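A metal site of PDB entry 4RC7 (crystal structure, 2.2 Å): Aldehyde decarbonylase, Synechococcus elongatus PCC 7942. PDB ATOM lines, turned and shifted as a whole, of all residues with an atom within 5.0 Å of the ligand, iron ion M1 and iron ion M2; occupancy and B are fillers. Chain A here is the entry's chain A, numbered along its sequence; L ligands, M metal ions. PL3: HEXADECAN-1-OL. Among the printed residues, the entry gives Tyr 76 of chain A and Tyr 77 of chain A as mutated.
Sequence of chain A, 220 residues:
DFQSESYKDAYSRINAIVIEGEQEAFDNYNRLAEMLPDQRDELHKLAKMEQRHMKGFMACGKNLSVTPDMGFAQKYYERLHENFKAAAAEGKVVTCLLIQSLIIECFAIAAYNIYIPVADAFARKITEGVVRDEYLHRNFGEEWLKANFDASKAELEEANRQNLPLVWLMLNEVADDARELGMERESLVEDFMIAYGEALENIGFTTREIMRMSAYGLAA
OE2 of Glu 134 touches iron ion M2, at 2.9 Å. Four residues have an atom within 4 Å of iron ion M2: Glu 22, Glu 50, His 53 and Glu 134.
OE2 of Glu 22 lies within hydrogen-bond range of OH of Tyr 112 (2.7 Å). OE1 of Glu 134 sits close to OE1 of Glu 105, at 2.7 Å. O of Gln 100 sits close to N of Glu 105 (3.3 Å). The side-chain carboxylate (OE2) of Glu 105 sits close to the side-chain hydroxyl (OH) of Tyr 29, 2.8 Å away. O of Ile 17 is in hydrogen-bond range of OH of Tyr 77, 2.8 Å away. The side-chain hydroxyl (OH) of Tyr 115 sits at hydrogen-bond distance from the side-chain hydroxyl (OH) of Tyr 11 (3.1 Å).
Iron ion M2 is bound by OE1 of Glu 22 (2.1 Å), OE1 of Glu 50 (2.1 Å) and ND1 of His 53 (2.4 Å).
The side-chain carboxylate (OE2) of Glu 50 binds iron ion M1 (2.1 Å). OE2 of Glu 105 binds iron ion M1. ND1 of His 137 is bound to iron ion M1 (2.3 Å). O1 of the ligand is bound to iron ion M1, 2.4 Å away. Iron ion M1 is bound by OE1 of Glu 105. Iron ion M1 has five donor atoms within binding distance.
Tyr 11 touches the ligand. CG2 of Ile 14 touches CC of the ligand, at 3.3 Å. Ile 17 touches the ligand. Val 18 touches the ligand. Gly 21 touches the ligand. Ala 25 touches the ligand (CB to O1, 3.6 Å). OH of Tyr 77 touches C5 of the ligand (3.2 Å). CG2 of Ile 104 touches C2 of the ligand, at 3.5 Å. CE2 of Phe 107 touches C8 of the ligand, 3.7 Å away. Ala 108 touches the ligand. CB of Ala 111 touches CB of the ligand (3.5 Å). Tyr 112 touches the ligand (OH to C3, 3.8 Å). Tyr 115 touches the ligand. Glu 134 touches the ligand. Of the 27 residues printed, 18 come within 4 Å of the ligand.
Glu 134 touches iron ion M1 (OE1 to FE, 3.8 Å). Four residues have an atom within 4 Å of iron ion M1: Glu 50, Glu 105, Glu 134 and His 137. The nearest printed residue that does not touch iron ion M1 is Tyr 29 (4.2 Å).
NE2 of Gln 100 sits close to O1 of the ligand (3.5 Å).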
ATOM      1  N   TYR A  11      16.747  -8.737  18.256  1.00  0.00           N
ATOM      2  CA  TYR A  11      15.731  -9.355  19.107  1.00  0.00           C
ATOM      3  C   TYR A  11      15.308  -8.426  20.224  1.00  0.00           C
ATOM      4  O   TYR A  11      14.192  -8.520  20.724  1.00  0.00           O
ATOM      5  CB  TYR A  11      16.214 -10.680  19.689  1.00  0.00           C
ATOM      6  CG  TYR A  11      15.073 -11.637  19.984  1.00  0.00           C
ATOM      7  CD1 TYR A  11      14.500 -12.402  18.974  1.00  0.00           C
ATOM      8  CD2 TYR A  11      14.603 -11.805  21.284  1.00  0.00           C
ATOM      9  CE1 TYR A  11      13.475 -13.294  19.240  1.00  0.00           C
ATOM     10  CE2 TYR A  11      13.560 -12.684  21.553  1.00  0.00           C
ATOM     11  CZ  TYR A  11      13.000 -13.434  20.529  1.00  0.00           C
ATOM     12  OH  TYR A  11      11.975 -14.322  20.786  1.00  0.00           O
ATOM     13  N   ILE A  14      12.504  -6.281  18.582  1.00  0.00           N
ATOM     14  CA  ILE A  14      11.382  -7.131  18.194  1.00  0.00           C
ATOM     15  C   ILE A  14      10.627  -7.665  19.405  1.00  0.00           C
ATOM     16  O   ILE A  14       9.413  -7.514  19.502  1.00  0.00           O
ATOM     17  CB  ILE A  14      11.818  -8.358  17.366  1.00  0.00           C
ATOM     18  CG1 ILE A  14      12.574  -7.919  16.115  1.00  0.00           C
ATOM     19  CG2 ILE A  14      10.612  -9.226  16.986  1.00  0.00           C
ATOM     20  CD1 ILE A  14      11.717  -7.198  15.119  1.00  0.00           C
ATOM     21  N   ILE A  17       8.738  -5.128  21.036  1.00  0.00           N
ATOM     22  CA  ILE A  17       7.552  -4.766  20.234  1.00  0.00           C
ATOM     23  C   ILE A  17       6.391  -5.714  20.443  1.00  0.00           C
ATOM     24  O   ILE A  17       5.237  -5.287  20.564  1.00  0.00           O
ATOM     25  CB  ILE A  17       7.894  -4.656  18.725  1.00  0.00           C
ATOM     26  CG1 ILE A  17       8.559  -3.298  18.447  1.00  0.00           C
ATOM     27  CG2 ILE A  17       6.659  -4.803  17.866  1.00  0.00           C
ATOM     28  CD1 ILE A  17       9.290  -3.248  17.105  1.00  0.00           C
ATOM     29  N   VAL A  18       6.675  -7.018  20.497  1.00  0.00           N
ATOM     30  CA  VAL A  18       5.610  -7.989  20.683  1.00  0.00           C
ATOM     31  C   VAL A  18       5.031  -7.908  22.081  1.00  0.00           C
ATOM     32  O   VAL A  18       3.819  -7.946  22.250  1.00  0.00           O
ATOM     33  CB  VAL A  18       6.005  -9.447  20.298  1.00  0.00           C
ATOM     34  CG1 VAL A  18       6.233  -9.537  18.794  1.00  0.00           C
ATOM     35  CG2 VAL A  18       7.255  -9.887  21.017  1.00  0.00           C
ATOM     36  N   GLY A  21       2.924  -4.833  22.301  1.00  0.00           N
ATOM     37  CA  GLY A  21       1.724  -5.104  21.501  1.00  0.00           C
ATOM     38  C   GLY A  21       0.693  -5.927  22.242  1.00  0.00           C
ATOM     39  O   GLY A  21      -0.500  -5.619  22.200  1.00  0.00           O
ATOM     40  N   GLU A  22       1.145  -6.978  22.927  1.00  0.00           N
ATOM     41  CA  GLU A  22       0.237  -7.844  23.681  1.00  0.00           C
ATOM     42  C   GLU A  22      -0.394  -7.078  24.844  1.00  0.00           C
ATOM     43  O   GLU A  22      -1.577  -7.234  25.139  1.00  0.00           O
ATOM     44  CB  GLU A  22       0.973  -9.084  24.197  1.00  0.00           C
ATOM     45  CG  GLU A  22       1.621  -9.922  23.113  1.00  0.00           C
ATOM     46  CD  GLU A  22       0.618 -10.600  22.175  1.00  0.00           C
ATOM     47  OE1 GLU A  22      -0.598 -10.621  22.460  1.00  0.00           O
ATOM     48  OE2 GLU A  22       1.064 -11.145  21.137  1.00  0.00           O
ATOM     49  N   ALA A  25      -2.956  -4.833  23.458  1.00  0.00           N
ATOM     50  CA  ALA A  25      -4.098  -5.683  23.080  1.00  0.00           C
ATOM     51  C   ALA A  25      -4.941  -6.008  24.319  1.00  0.00           C
ATOM     52  O   ALA A  25      -6.174  -5.934  24.295  1.00  0.00           O
ATOM     53  CB  ALA A  25      -3.627  -6.951  22.378  1.00  0.00           C
ATOM     54  N   TYR A  29      -8.898  -4.727  24.482  1.00  0.00           N
ATOM     55  CA  TYR A  29     -10.061  -5.623  24.573  1.00  0.00           C
ATOM     56  C   TYR A  29     -10.862  -5.373  25.853  1.00  0.00           C
ATOM     57  O   TYR A  29     -12.096  -5.500  25.830  1.00  0.00           O
ATOM     58  CB  TYR A  29      -9.665  -7.103  24.440  1.00  0.00           C
ATOM     59  CG  TYR A  29      -9.407  -7.534  23.011  1.00  0.00           C
ATOM     60  CD1 TYR A  29     -10.380  -7.401  22.040  1.00  0.00           C
ATOM     61  CD2 TYR A  29      -8.186  -8.100  22.640  1.00  0.00           C
ATOM     62  CE1 TYR A  29     -10.152  -7.791  20.736  1.00  0.00           C
ATOM     63  CE2 TYR A  29      -7.941  -8.508  21.341  1.00  0.00           C
ATOM     64  CZ  TYR A  29      -8.918  -8.349  20.390  1.00  0.00           C
ATOM     65  OH  TYR A  29      -8.693  -8.752  19.092  1.00  0.00           O
ATOM     66  N   GLU A  50      -4.601 -12.275  25.804  1.00  0.00           N
ATOM     67  CA  GLU A  50      -3.505 -11.338  25.530  1.00  0.00           C
ATOM     68  C   GLU A  50      -2.469 -11.287  26.683  1.00  0.00           C
ATOM     69  O   GLU A  50      -1.256 -11.285  26.444  1.00  0.00           O
ATOM     70  CB  GLU A  50      -4.028  -9.931  25.209  1.00  0.00           C
ATOM     71  CG  GLU A  50      -5.060  -9.872  24.082  1.00  0.00           C
ATOM     72  CD  GLU A  50      -4.535 -10.301  22.717  1.00  0.00           C
ATOM     73  OE1 GLU A  50      -3.382 -10.786  22.626  1.00  0.00           O
ATOM     74  OE2 GLU A  50      -5.282 -10.166  21.730  1.00  0.00           O
ATOM     75  N   HIS A  53      -0.175 -14.194  26.318  1.00  0.00           N
ATOM     76  CA  HIS A  53       0.797 -13.951  25.250  1.00  0.00           C
ATOM     77  C   HIS A  53       1.926 -13.074  25.726  1.00  0.00           C
ATOM     78  O   HIS A  53       3.089 -13.352  25.462  1.00  0.00           O
ATOM     79  CB  HIS A  53       0.105 -13.300  24.050  1.00  0.00           C
ATOM     80  CG  HIS A  53      -1.028 -14.093  23.490  1.00  0.00           C
ATOM     81  ND1 HIS A  53      -1.861 -13.602  22.572  1.00  0.00           N
ATOM     82  CD2 HIS A  53      -1.456 -15.397  23.753  1.00  0.00           C
ATOM     83  CE1 HIS A  53      -2.783 -14.532  22.240  1.00  0.00           C
ATOM     84  NE2 HIS A  53      -2.534 -15.629  22.979  1.00  0.00           N
ATOM     85  N   PHE A  57       5.927 -14.117  25.732  1.00  0.00           N
ATOM     86  CA  PHE A  57       6.999 -13.445  25.006  1.00  0.00           C
ATOM     87  C   PHE A  57       8.052 -12.816  25.905  1.00  0.00           C
ATOM     88  O   PHE A  57       9.207 -12.687  25.509  1.00  0.00           O
ATOM     89  CB  PHE A  57       6.438 -12.438  24.022  1.00  0.00           C
ATOM     90  CG  PHE A  57       5.734 -13.087  22.867  1.00  0.00           C
ATOM     91  CD1 PHE A  57       6.432 -13.950  22.017  1.00  0.00           C
ATOM     92  CD2 PHE A  57       4.380 -12.844  22.623  1.00  0.00           C
ATOM     93  CE1 PHE A  57       5.792 -14.545  20.933  1.00  0.00           C
ATOM     94  CE2 PHE A  57       3.748 -13.449  21.558  1.00  0.00           C
ATOM     95  CZ  PHE A  57       4.458 -14.305  20.711  1.00  0.00           C
ATOM     96  N   TYR A  76       6.978   3.004  19.001  1.00  0.00           N
ATOM     97  CA  TYR A  76       6.525   2.242  17.849  1.00  0.00           C
ATOM     98  C   TYR A  76       5.001   2.250  17.743  1.00  0.00           C
ATOM     99  O   TYR A  76       4.458   2.487  16.672  1.00  0.00           O
ATOM    100  CB  TYR A  76       7.017   0.806  17.970  1.00  0.00           C
ATOM    101  CG  TYR A  76       6.799  -0.101  16.773  1.00  0.00           C
ATOM    102  CD1 TYR A  76       7.551   0.033  15.610  1.00  0.00           C
ATOM    103  CD2 TYR A  76       5.873  -1.131  16.846  1.00  0.00           C
ATOM    104  CE1 TYR A  76       7.383  -0.841  14.540  1.00  0.00           C
ATOM    105  CE2 TYR A  76       5.685  -2.004  15.785  1.00  0.00           C
ATOM    106  CZ  TYR A  76       6.448  -1.871  14.644  1.00  0.00           C
ATOM    107  OH  TYR A  76       6.232  -2.733  13.597  1.00  0.00           O
ATOM    108  N   TYR A  77       4.330   2.024  18.873  1.00  0.00           N
ATOM    109  CA  TYR A  77       2.873   1.907  18.914  1.00  0.00           C
ATOM    110  C   TYR A  77       2.113   3.205  19.140  1.00  0.00           C
ATOM    111  O   TYR A  77       0.900   3.245  18.929  1.00  0.00           O
ATOM    112  CB  TYR A  77       2.466   0.912  20.008  1.00  0.00           C
ATOM    113  CG  TYR A  77       2.667  -0.549  19.652  1.00  0.00           C
ATOM    114  CD1 TYR A  77       1.704  -1.251  18.924  1.00  0.00           C
ATOM    115  CD2 TYR A  77       3.820  -1.216  20.049  1.00  0.00           C
ATOM    116  CE1 TYR A  77       1.888  -2.600  18.603  1.00  0.00           C
ATOM    117  CE2 TYR A  77       4.007  -2.556  19.754  1.00  0.00           C
ATOM    118  CZ  TYR A  77       3.037  -3.243  19.022  1.00  0.00           C
ATOM    119  OH  TYR A  77       3.247  -4.574  18.721  1.00  0.00           O
ATOM    120  N   GLN A 100      -7.902  -2.886  16.526  1.00  0.00           N
ATOM    121  CA  GLN A 100      -7.386  -4.029  17.286  1.00  0.00           C
ATOM    122  C   GLN A 100      -7.713  -5.401  16.667  1.00  0.00           C
ATOM    123  O   GLN A 100      -6.814  -6.195  16.470  1.00  0.00           O
ATOM    124  CB  GLN A 100      -7.807  -3.982  18.757  1.00  0.00           C
ATOM    125  CG  GLN A 100      -7.359  -5.208  19.563  1.00  0.00           C
ATOM    126  CD  GLN A 100      -5.844  -5.350  19.622  1.00  0.00           C
ATOM    127  OE1 GLN A 100      -5.132  -4.398  19.937  1.00  0.00           O
ATOM    128  NE2 GLN A 100      -5.349  -6.545  19.323  1.00  0.00           N
ATOM    129  N   ILE A 104      -4.552  -4.881  13.586  1.00  0.00           N
ATOM    130  CA  ILE A 104      -3.480  -5.395  14.436  1.00  0.00           C
ATOM    131  C   ILE A 104      -3.390  -6.931  14.431  1.00  0.00           C
ATOM    132  O   ILE A 104      -2.293  -7.479  14.309  1.00  0.00           O
ATOM    133  CB  ILE A 104      -3.570  -4.853  15.880  1.00  0.00           C
ATOM    134  CG1 ILE A 104      -3.177  -3.363  15.921  1.00  0.00           C
ATOM    135  CG2 ILE A 104      -2.612  -5.618  16.799  1.00  0.00           C
ATOM    136  CD1 ILE A 104      -3.385  -2.694  17.291  1.00  0.00           C
ATOM    137  N   GLU A 105      -4.518  -7.621  14.568  1.00  0.00           N
ATOM    138  CA  GLU A 105      -4.477  -9.096  14.553  1.00  0.00           C
ATOM    139  C   GLU A 105      -3.944  -9.635  13.230  1.00  0.00           C
ATOM    140  O   GLU A 105      -3.183 -10.567  13.236  1.00  0.00           O
ATOM    141  CB  GLU A 105      -5.845  -9.726  14.852  1.00  0.00           C
ATOM    142  CG  GLU A 105      -6.460  -9.383  16.206  1.00  0.00           C
ATOM    143  CD  GLU A 105      -5.696  -9.935  17.398  1.00  0.00           C
ATOM    144  OE1 GLU A 105      -4.799 -10.791  17.240  1.00  0.00           O
ATOM    145  OE2 GLU A 105      -6.032  -9.505  18.515  1.00  0.00           O
ATOM    146  N   PHE A 107      -1.876  -8.208  11.251  1.00  0.00           N
ATOM    147  CA  PHE A 107      -0.452  -7.914  11.228  1.00  0.00           C
ATOM    148  C   PHE A 107       0.291  -8.959  12.057  1.00  0.00           C
ATOM    149  O   PHE A 107       1.290  -9.506  11.602  1.00  0.00           O
ATOM    150  CB  PHE A 107      -0.221  -6.506  11.790  1.00  0.00           C
ATOM    151  CG  PHE A 107       1.212  -6.020  11.707  1.00  0.00           C
ATOM    152  CD1 PHE A 107       2.014  -6.333  10.619  1.00  0.00           C
ATOM    153  CD2 PHE A 107       1.727  -5.193  12.706  1.00  0.00           C
ATOM    154  CE1 PHE A 107       3.318  -5.874  10.537  1.00  0.00           C
ATOM    155  CE2 PHE A 107       3.032  -4.729  12.638  1.00  0.00           C
ATOM    156  CZ  PHE A 107       3.827  -5.073  11.547  1.00  0.00           C
ATOM    157  N   ALA A 108      -0.204  -9.229  13.246  1.00  0.00           N
ATOM    158  CA  ALA A 108       0.385 -10.233  14.135  1.00  0.00           C
ATOM    159  C   ALA A 108       0.360 -11.628  13.518  1.00  0.00           C
ATOM    160  O   ALA A 108       1.342 -12.345  13.556  1.00  0.00           O
ATOM    161  CB  ALA A 108      -0.325 -10.232  15.479  1.00  0.00           C
ATOM    162  N   ALA A 111       3.059 -11.805  10.707  1.00  0.00           N
ATOM    163  CA  ALA A 111       4.429 -11.765  11.236  1.00  0.00           C
ATOM    164  C   ALA A 111       4.773 -13.002  12.095  1.00  0.00           C
ATOM    165  O   ALA A 111       5.866 -13.525  12.017  1.00  0.00           O
ATOM    166  CB  ALA A 111       4.665 -10.500  12.042  1.00  0.00           C
ATOM    167  N   TYR A 112       3.834 -13.450  12.927  1.00  0.00           N
ATOM    168  CA  TYR A 112       4.098 -14.583  13.792  1.00  0.00           C
ATOM    169  C   TYR A 112       4.278 -15.861  12.956  1.00  0.00           C
ATOM    170  O   TYR A 112       5.175 -16.660  13.225  1.00  0.00           O
ATOM    171  CB  TYR A 112       2.974 -14.769  14.809  1.00  0.00           C
ATOM    172  CG  TYR A 112       2.917 -13.753  15.923  1.00  0.00           C
ATOM    173  CD1 TYR A 112       3.944 -12.848  16.132  1.00  0.00           C
ATOM    174  CD2 TYR A 112       1.837 -13.715  16.787  1.00  0.00           C
ATOM    175  CE1 TYR A 112       3.889 -11.912  17.147  1.00  0.00           C
ATOM    176  CE2 TYR A 112       1.771 -12.785  17.821  1.00  0.00           C
ATOM    177  CZ  TYR A 112       2.806 -11.887  17.994  1.00  0.00           C
ATOM    178  OH  TYR A 112       2.749 -10.960  19.006  1.00  0.00           O
ATOM    179  N   TYR A 115       7.645 -15.820  11.538  1.00  0.00           N
ATOM    180  CA  TYR A 115       8.670 -16.045  12.540  1.00  0.00           C
ATOM    181  C   TYR A 115       8.810 -17.522  12.934  1.00  0.00           C
ATOM    182  O   TYR A 115       9.910 -17.996  13.171  1.00  0.00           O
ATOM    183  CB  TYR A 115       8.376 -15.192  13.764  1.00  0.00           C
ATOM    184  CG  TYR A 115       9.315 -15.403  14.929  1.00  0.00           C
ATOM    185  CD1 TYR A 115      10.695 -15.207  14.795  1.00  0.00           C
ATOM    186  CD2 TYR A 115       8.818 -15.784  16.169  1.00  0.00           C
ATOM    187  CE1 TYR A 115      11.546 -15.391  15.867  1.00  0.00           C
ATOM    188  CE2 TYR A 115       9.659 -15.970  17.250  1.00  0.00           C
ATOM    189  CZ  TYR A 115      11.020 -15.761  17.099  1.00  0.00           C
ATOM    190  OH  TYR A 115      11.849 -15.954  18.176  1.00  0.00           O
ATOM    191  N   THR A 127       5.109 -19.273  20.212  1.00  0.00           N
ATOM    192  CA  THR A 127       4.468 -18.496  19.156  1.00  0.00           C
ATOM    193  C   THR A 127       3.369 -19.312  18.502  1.00  0.00           C
ATOM    194  O   THR A 127       2.311 -18.782  18.216  1.00  0.00           O
ATOM    195  CB  THR A 127       5.496 -17.994  18.104  1.00  0.00           C
ATOM    196  OG1 THR A 127       6.551 -17.291  18.784  1.00  0.00           O
ATOM    197  CG2 THR A 127       4.826 -17.020  17.098  1.00  0.00           C
ATOM    198  N   VAL A 130       0.466 -18.922  20.605  1.00  0.00           N
ATOM    199  CA  VAL A 130      -0.025 -17.575  20.457  1.00  0.00           C
ATOM    200  C   VAL A 130      -0.833 -17.408  19.174  1.00  0.00           C
ATOM    201  O   VAL A 130      -1.968 -16.935  19.207  1.00  0.00           O
ATOM    202  CB  VAL A 130       1.139 -16.547  20.521  1.00  0.00           C
ATOM    203  CG1 VAL A 130       0.716 -15.180  20.015  1.00  0.00           C
ATOM    204  CG2 VAL A 130       1.622 -16.430  21.956  1.00  0.00           C
ATOM    205  N   GLU A 134      -4.724 -15.800  18.032  1.00  0.00           N
ATOM    206  CA  GLU A 134      -4.895 -14.656  17.146  1.00  0.00           C
ATOM    207  C   GLU A 134      -5.990 -14.895  16.094  1.00  0.00           C
ATOM    208  O   GLU A 134      -6.774 -13.994  15.789  1.00  0.00           O
ATOM    209  CB  GLU A 134      -3.566 -14.221  16.500  1.00  0.00           C
ATOM    210  CG  GLU A 134      -2.387 -14.202  17.475  1.00  0.00           C
ATOM    211  CD  GLU A 134      -1.875 -12.807  17.823  1.00  0.00           C
ATOM    212  OE1 GLU A 134      -2.313 -11.830  17.172  1.00  0.00           O
ATOM    213  OE2 GLU A 134      -1.029 -12.668  18.748  1.00  0.00           O
ATOM    214  N   HIS A 137      -9.270 -14.076  17.721  1.00  0.00           N
ATOM    215  CA  HIS A 137      -9.438 -12.640  17.939  1.00  0.00           C
ATOM    216  C   HIS A 137      -9.867 -11.949  16.666  1.00  0.00           C
ATOM    217  O   HIS A 137     -10.790 -11.151  16.667  1.00  0.00           O
ATOM    218  CB  HIS A 137      -8.130 -12.025  18.436  1.00  0.00           C
ATOM    219  CG  HIS A 137      -7.637 -12.562  19.757  1.00  0.00           C
ATOM    220  ND1 HIS A 137      -6.516 -12.113  20.344  1.00  0.00           N
ATOM    221  CD2 HIS A 137      -8.152 -13.563  20.590  1.00  0.00           C
ATOM    222  CE1 HIS A 137      -6.315 -12.809  21.489  1.00  0.00           C
ATOM    223  NE2 HIS A 137      -7.317 -13.676  21.636  1.00  0.00           N
ATOM    224  N   VAL A 174       9.998  -1.980  11.171  1.00  0.00           N
ATOM    225  CA  VAL A 174      10.448  -3.227  11.773  1.00  0.00           C
ATOM    226  C   VAL A 174      11.219  -4.119  10.773  1.00  0.00           C
ATOM    227  O   VAL A 174      11.830  -5.120  11.165  1.00  0.00           O
ATOM    228  CB  VAL A 174       9.269  -3.966  12.452  1.00  0.00           C
ATOM    229  CG1 VAL A 174       8.537  -4.906  11.488  1.00  0.00           C
ATOM    230  CG2 VAL A 174       9.768  -4.708  13.675  1.00  0.00           C
ATOM    231  N   MET A 183      13.465 -13.148   8.834  1.00  0.00           N
ATOM    232  CA  MET A 183      12.127 -12.945   8.269  1.00  0.00           C
ATOM    233  C   MET A 183      12.192 -11.960   7.092  1.00  0.00           C
ATOM    234  O   MET A 183      12.530 -10.786   7.268  1.00  0.00           O
ATOM    235  CB  MET A 183      11.182 -12.393   9.340  1.00  0.00           C
ATOM    236  CG  MET A 183      11.127 -13.242  10.609  1.00  0.00           C
ATOM    237  SD  MET A 183      10.224 -12.476  11.959  1.00  0.00           S
ATOM    238  CE  MET A 183      11.290 -11.128  12.435  1.00  0.00           C
HETATM  239  C1  PL3 L   1      -1.763  -9.021  19.627  1.00  0.00           C
HETATM  240  O1  PL3 L   1      -2.994  -9.121  19.518  1.00  0.00           O
HETATM  241  C2  PL3 L   1      -1.104  -7.804  19.016  1.00  0.00           C
HETATM  242  C3  PL3 L   1       0.396  -7.997  18.845  1.00  0.00           C
HETATM  243  C4  PL3 L   1       0.899  -7.257  17.596  1.00  0.00           C
HETATM  244  C5  PL3 L   1       2.438  -7.414  17.476  1.00  0.00           C
HETATM  245  C6  PL3 L   1       2.882  -7.259  16.016  1.00  0.00           C
HETATM  246  C7  PL3 L   1       4.401  -7.039  15.936  1.00  0.00           C
HETATM  247  C8  PL3 L   1       4.949  -7.265  14.528  1.00  0.00           C
HETATM  248  C9  PL3 L   1       6.431  -6.881  14.449  1.00  0.00           C
HETATM  249  CA  PL3 L   1       7.393  -8.046  14.175  1.00  0.00           C
HETATM  250  CB  PL3 L   1       6.850  -9.420  14.554  1.00  0.00           C
HETATM  251  CC  PL3 L   1       7.816 -10.193  15.437  1.00  0.00           C
HETATM  252  CD  PL3 L   1       7.507 -11.685  15.510  1.00  0.00           C
HETATM  253  CE  PL3 L   1       8.509 -12.344  16.445  1.00  0.00           C
HETATM  254  CF  PL3 L   1       7.897 -12.651  17.828  1.00  0.00           C
HETATM  255  CG  PL3 L   1       9.007 -12.772  18.880  1.00  0.00           C
HETATM  256 FE    FE M   1      -4.767 -10.736  19.803  1.00  0.00          FE
HETATM  257 FE    FE M   2      -1.970 -11.611  21.276  1.00  0.00          FE
